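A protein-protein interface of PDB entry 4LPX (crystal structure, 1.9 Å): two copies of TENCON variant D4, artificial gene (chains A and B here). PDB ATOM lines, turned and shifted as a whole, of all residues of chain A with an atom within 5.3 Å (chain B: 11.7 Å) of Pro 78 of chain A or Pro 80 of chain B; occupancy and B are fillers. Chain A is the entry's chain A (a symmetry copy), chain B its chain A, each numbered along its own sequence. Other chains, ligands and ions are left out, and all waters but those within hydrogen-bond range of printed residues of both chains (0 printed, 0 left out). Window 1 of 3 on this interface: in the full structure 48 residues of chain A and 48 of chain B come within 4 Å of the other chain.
The backbone NH of Asp 30 of chain B is in hydrogen-bond range of the backbone carbonyl oxygen of Val 75 of chain B, 2.9 Å away.
Val 75 of chain A touches Pro 80 of chain B, and with the chains exchanged Pro 80 of chain A touches Val 75 of chain B.
Leu 76 of chain A touches Pro 80 of chain B, and with the chains exchanged Pro 80 of chain A touches Leu 76 of chain B.
Pro 78 of chain A touches Pro 80 of chain B, and with the chains exchanged Pro 80 of chain A touches Pro 78 of chain B.
Positions printed for both chains: 75, 76, 77, 78, 79 and 80.
The backbone carbonyl oxygen (O) of Asn 81 of chain B lies within hydrogen-bond range of the backbone NH (N) of Leu 76 of chain A (2.8 Å).
Val 75 of chain A touches just these residues of chain B: Pro 80 (3.9 Å), Asn 81 (3.4 Å) and Leu 82 (3.7 Å).
No residue of chain B comes within 4 Å of Ile 77 of chain A.
Of the printed residues of chain A, Val 75 of chain B touches Pro 80.
Of the printed residues of chain A, Pro 78 of chain B touches Pro 80.
Of chain A, only Val 75 (3.9 Å), Leu 76 (3.6 Å) and Pro 78 (3.9 Å) come within 4 Å of Pro 80 of chain B.
Printed residues of chain A within 4 Å of Leu 82 of chain B: Val 75.
The nearest printed residue of chain A that does not touch Pro 78 of chain B is Phe 79 of chain A (4.001 Å).
Of the 6 printed residues of chain A, 4 touch a printed residue of chain B.
Hydrophobic or aromatic side chains of chain A that line the printed part of chain B: Val 75, Leu 76, Pro 78 and Pro 80.
Along chain A the printed residues that touch a printed residue of chain B span positions 75 to 80.
Val 75 of chain A touches Pro 80 of chain B (CG1 to CB, 3.9 Å).
Val 75 of chain A touches Asn 81 of chain B (CA to O, 3.4 Å).
CG2 of Val 75 of chain A touches CD2 of Leu 82 of chain B (3.7 Å).
Leu 76 of chain A touches Pro 80 of chain B (O to CA, 3.6 Å).
CD of Pro 78 of chain A touches CA of Pro 80 of chain B (3.9 Å).
Pro 78 of chain A touches Asn 81 of chain B (CG to ND2, 3.9 Å).
CB of Pro 80 of chain A touches CG1 of Val 75 of chain B, at 3.9 Å.
Pro 80 of chain A touches Leu 76 of chain B.
Pro 78 of chain B touches Pro 80 of chain A.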
ATOM      1  N   VAL A  75     -23.949  -6.228  26.414  1.00  0.00           N
ATOM      2  CA  VAL A  75     -24.133  -4.771  26.374  1.00  0.00           C
ATOM      3  C   VAL A  75     -23.649  -4.199  27.707  1.00  0.00           C
ATOM      4  O   VAL A  75     -24.018  -4.704  28.763  1.00  0.00           O
ATOM      5  CB  VAL A  75     -25.623  -4.411  26.170  1.00  0.00           C
ATOM      6  CG1 VAL A  75     -25.857  -2.875  26.126  1.00  0.00           C
ATOM      7  CG2 VAL A  75     -26.165  -5.053  24.863  1.00  0.00           C
ATOM      8  N   LEU A  76     -22.828  -3.151  27.651  1.00  0.00           N
ATOM      9  CA  LEU A  76     -22.392  -2.439  28.865  1.00  0.00           C
ATOM     10  C   LEU A  76     -22.791  -0.977  28.683  1.00  0.00           C
ATOM     11  O   LEU A  76     -22.378  -0.356  27.719  1.00  0.00           O
ATOM     12  CB  LEU A  76     -20.866  -2.547  29.029  1.00  0.00           C
ATOM     13  CG  LEU A  76     -20.205  -2.127  30.360  1.00  0.00           C
ATOM     14  CD1 LEU A  76     -20.234  -0.600  30.617  1.00  0.00           C
ATOM     15  CD2 LEU A  76     -20.791  -2.890  31.546  1.00  0.00           C
ATOM     16  N   ILE A  77     -23.587  -0.446  29.603  1.00  0.00           N
ATOM     17  CA  ILE A  77     -24.030   0.948  29.547  1.00  0.00           C
ATOM     18  C   ILE A  77     -23.077   1.833  30.394  1.00  0.00           C
ATOM     19  O   ILE A  77     -23.101   1.761  31.622  1.00  0.00           O
ATOM     20  CB  ILE A  77     -25.492   1.086  30.010  1.00  0.00           C
ATOM     21  CG1 ILE A  77     -26.414   0.192  29.138  1.00  0.00           C
ATOM     22  CG2 ILE A  77     -25.944   2.582  29.983  1.00  0.00           C
ATOM     23  CD1 ILE A  77     -27.828   0.102  29.639  1.00  0.00           C
ATOM     24  N   PRO A  78     -22.242   2.661  29.731  1.00  0.00           N
ATOM     25  CA  PRO A  78     -21.281   3.470  30.510  1.00  0.00           C
ATOM     26  C   PRO A  78     -21.972   4.582  31.287  1.00  0.00           C
ATOM     27  O   PRO A  78     -23.067   5.026  30.907  1.00  0.00           O
ATOM     28  CB  PRO A  78     -20.355   4.087  29.444  1.00  0.00           C
ATOM     29  CG  PRO A  78     -20.791   3.555  28.118  1.00  0.00           C
ATOM     30  CD  PRO A  78     -22.134   2.901  28.277  1.00  0.00           C
ATOM     31  N   PHE A  79     -21.341   5.030  32.367  1.00  0.00           N
ATOM     32  CA  PHE A  79     -21.804   6.217  33.073  1.00  0.00           C
ATOM     33  C   PHE A  79     -21.692   7.421  32.112  1.00  0.00           C
ATOM     34  O   PHE A  79     -20.757   7.492  31.307  1.00  0.00           O
ATOM     35  CB  PHE A  79     -20.976   6.446  34.348  1.00  0.00           C
ATOM     36  CG  PHE A  79     -21.582   7.469  35.261  1.00  0.00           C
ATOM     37  CD1 PHE A  79     -22.687   7.155  36.034  1.00  0.00           C
ATOM     38  CD2 PHE A  79     -21.037   8.748  35.338  1.00  0.00           C
ATOM     39  CE1 PHE A  79     -23.251   8.096  36.878  1.00  0.00           C
ATOM     40  CE2 PHE A  79     -21.591   9.703  36.179  1.00  0.00           C
ATOM     41  CZ  PHE A  79     -22.702   9.372  36.950  1.00  0.00           C
ATOM     42  N   PRO A  80     -22.640   8.377  32.182  1.00  0.00           N
ATOM     43  CA  PRO A  80     -22.484   9.560  31.317  1.00  0.00           C
ATOM     44  C   PRO A  80     -21.191  10.355  31.560  1.00  0.00           C
ATOM     45  O   PRO A  80     -20.650  10.350  32.672  1.00  0.00           O
ATOM     46  CB  PRO A  80     -23.721  10.410  31.652  1.00  0.00           C
ATOM     47  CG  PRO A  80     -24.706   9.429  32.178  1.00  0.00           C
ATOM     48  CD  PRO A  80     -23.875   8.455  32.978  1.00  0.00           C
ATOM     49  N   ASP B  30     -25.986  16.404  25.515  1.00  0.00           N
ATOM     50  CA  ASP B  30     -27.314  15.791  25.553  1.00  0.00           C
ATOM     51  C   ASP B  30     -28.208  16.441  26.597  1.00  0.00           C
ATOM     52  O   ASP B  30     -29.416  16.532  26.413  1.00  0.00           O
ATOM     53  CB  ASP B  30     -27.208  14.302  25.866  1.00  0.00           C
ATOM     54  CG  ASP B  30     -26.535  13.535  24.745  1.00  0.00           C
ATOM     55  OD1 ASP B  30     -27.082  13.538  23.620  1.00  0.00           O
ATOM     56  OD2 ASP B  30     -25.467  12.938  24.989  1.00  0.00           O
ATOM     57  N   VAL B  75     -23.617  17.311  30.025  1.00  0.00           N
ATOM     58  CA  VAL B  75     -23.740  15.851  30.119  1.00  0.00           C
ATOM     59  C   VAL B  75     -23.722  15.284  28.698  1.00  0.00           C
ATOM     60  O   VAL B  75     -24.437  15.776  27.831  1.00  0.00           O
ATOM     61  CB  VAL B  75     -25.066  15.454  30.812  1.00  0.00           C
ATOM     62  CG1 VAL B  75     -25.233  13.914  30.926  1.00  0.00           C
ATOM     63  CG2 VAL B  75     -25.150  16.089  32.228  1.00  0.00           C
ATOM     64  N   LEU B  76     -22.904  14.256  28.469  1.00  0.00           N
ATOM     65  CA  LEU B  76     -22.886  13.550  27.176  1.00  0.00           C
ATOM     66  C   LEU B  76     -23.165  12.080  27.477  1.00  0.00           C
ATOM     67  O   LEU B  76     -22.436  11.474  28.241  1.00  0.00           O
ATOM     68  CB  LEU B  76     -21.508  13.695  26.506  1.00  0.00           C
ATOM     69  CG  LEU B  76     -21.325  13.285  25.030  1.00  0.00           C
ATOM     70  CD1 LEU B  76     -21.402  11.758  24.791  1.00  0.00           C
ATOM     71  CD2 LEU B  76     -22.296  14.029  24.114  1.00  0.00           C
ATOM     72  N   ILE B  77     -24.212  11.526  26.876  1.00  0.00           N
ATOM     73  CA  ILE B  77     -24.575  10.123  27.073  1.00  0.00           C
ATOM     74  C   ILE B  77     -23.943   9.257  25.950  1.00  0.00           C
ATOM     75  O   ILE B  77     -24.382   9.323  24.803  1.00  0.00           O
ATOM     76  CB  ILE B  77     -26.104   9.947  27.130  1.00  0.00           C
ATOM     77  CG1 ILE B  77     -26.699  10.821  28.266  1.00  0.00           C
ATOM     78  CG2 ILE B  77     -26.484   8.441  27.302  1.00  0.00           C
ATOM     79  CD1 ILE B  77     -28.201  10.875  28.272  1.00  0.00           C
ATOM     80  N   PRO B  78     -22.912   8.452  26.289  1.00  0.00           N
ATOM     81  CA  PRO B  78     -22.252   7.664  25.227  1.00  0.00           C
ATOM     82  C   PRO B  78     -23.138   6.532  24.726  1.00  0.00           C
ATOM     83  O   PRO B  78     -24.029   6.063  25.450  1.00  0.00           O
ATOM     84  CB  PRO B  78     -21.006   7.075  25.916  1.00  0.00           C
ATOM     85  CG  PRO B  78     -20.980   7.601  27.314  1.00  0.00           C
ATOM     86  CD  PRO B  78     -22.315   8.221  27.620  1.00  0.00           C
ATOM     87  N   PHE B  79     -22.896   6.094  23.493  1.00  0.00           N
ATOM     88  CA  PHE B  79     -23.542   4.894  22.981  1.00  0.00           C
ATOM     89  C   PHE B  79     -23.083   3.697  23.841  1.00  0.00           C
ATOM     90  O   PHE B  79     -21.930   3.653  24.284  1.00  0.00           O
ATOM     91  CB  PHE B  79     -23.189   4.679  21.499  1.00  0.00           C
ATOM     92  CG  PHE B  79     -24.041   3.639  20.840  1.00  0.00           C
ATOM     93  CD1 PHE B  79     -25.350   3.923  20.486  1.00  0.00           C
ATOM     94  CD2 PHE B  79     -23.524   2.373  20.578  1.00  0.00           C
ATOM     95  CE1 PHE B  79     -26.142   2.965  19.879  1.00  0.00           C
ATOM     96  CE2 PHE B  79     -24.305   1.401  19.970  1.00  0.00           C
ATOM     97  CZ  PHE B  79     -25.619   1.702  19.620  1.00  0.00           C
ATOM     98  N   PRO B  80     -23.976   2.718  24.092  1.00  0.00           N
ATOM     99  CA  PRO B  80     -23.508   1.543  24.848  1.00  0.00           C
ATOM    100  C   PRO B  80     -22.355   0.778  24.179  1.00  0.00           C
ATOM    101  O   PRO B  80     -22.221   0.793  22.951  1.00  0.00           O
ATOM    102  CB  PRO B  80     -24.764   0.662  24.948  1.00  0.00           C
ATOM    103  CG  PRO B  80     -25.893   1.616  24.788  1.00  0.00           C
ATOM    104  CD  PRO B  80     -25.405   2.606  23.760  1.00  0.00           C
ATOM    105  N   ASN B  81     -21.537   0.120  25.000  1.00  0.00           N
ATOM    106  CA  ASN B  81     -20.474  -0.757  24.514  1.00  0.00           C
ATOM    107  C   ASN B  81     -21.113  -2.108  24.197  1.00  0.00           C
ATOM    108  O   ASN B  81     -21.861  -2.634  25.022  1.00  0.00           O
ATOM    109  CB  ASN B  81     -19.406  -0.958  25.607  1.00  0.00           C
ATOM    110  CG  ASN B  81     -18.755   0.355  26.068  1.00  0.00           C
ATOM    111  OD1 ASN B  81     -18.439   1.229  25.261  1.00  0.00           O
ATOM    112  ND2 ASN B  81     -18.555   0.486  27.377  1.00  0.00           N
ATOM    113  N   LEU B  82     -20.820  -2.653  23.019  1.00  0.00           N
ATOM    114  CA  LEU B  82     -21.295  -3.983  22.611  1.00  0.00           C
ATOM    115  C   LEU B  82     -20.113  -4.934  22.520  1.00  0.00           C
ATOM    116  O   LEU B  82     -19.025  -4.533  22.085  1.00  0.00           O
ATOM    117  CB  LEU B  82     -21.953  -3.935  21.232  1.00  0.00           C
ATOM    118  CG  LEU B  82     -23.415  -3.606  20.953  1.00  0.00           C
ATOM    119  CD1 LEU B  82     -23.667  -3.730  19.461  1.00  0.00           C
ATOM    120  CD2 LEU B  82     -24.376  -4.515  21.710  1.00  0.00           C
ATOM    121  N   SER B  83     -20.310  -6.189  22.924  1.00  0.00           N
ATOM    122  CA  SER B  83     -19.319  -7.232  22.649  1.00  0.00           C
ATOM    123  C   SER B  83     -19.381  -7.610  21.168  1.00  0.00           C
ATOM    124  O   SER B  83     -20.278  -7.179  20.432  1.00  0.00           O
ATOM    125  CB  SER B  83     -19.592  -8.467  23.508  1.00  0.00           C
ATOM    126  OG  SER B  83     -20.755  -9.138  23.032  1.00  0.00           O
ATOM    127  N   ASN B  84     -18.425  -8.417  20.718  1.00  0.00           N
ATOM    128  CA  ASN B  84     -18.598  -9.153  19.469  1.00  0.00           C
ATOM    129  C   ASN B  84     -19.854 -10.041  19.574  1.00  0.00           C
ATOM    130  O   ASN B  84     -20.166 -10.527  20.661  1.00  0.00           O
ATOM    131  CB  ASN B  84     -17.367 -10.025  19.189  1.00  0.00           C
ATOM    132  CG  ASN B  84     -16.156  -9.212  18.760  1.00  0.00           C
ATOM    133  OD1 ASN B  84     -16.257  -8.319  17.910  1.00  0.00           O
ATOM    134  ND2 ASN B  84     -15.004  -9.518  19.348  1.00  0.00           N
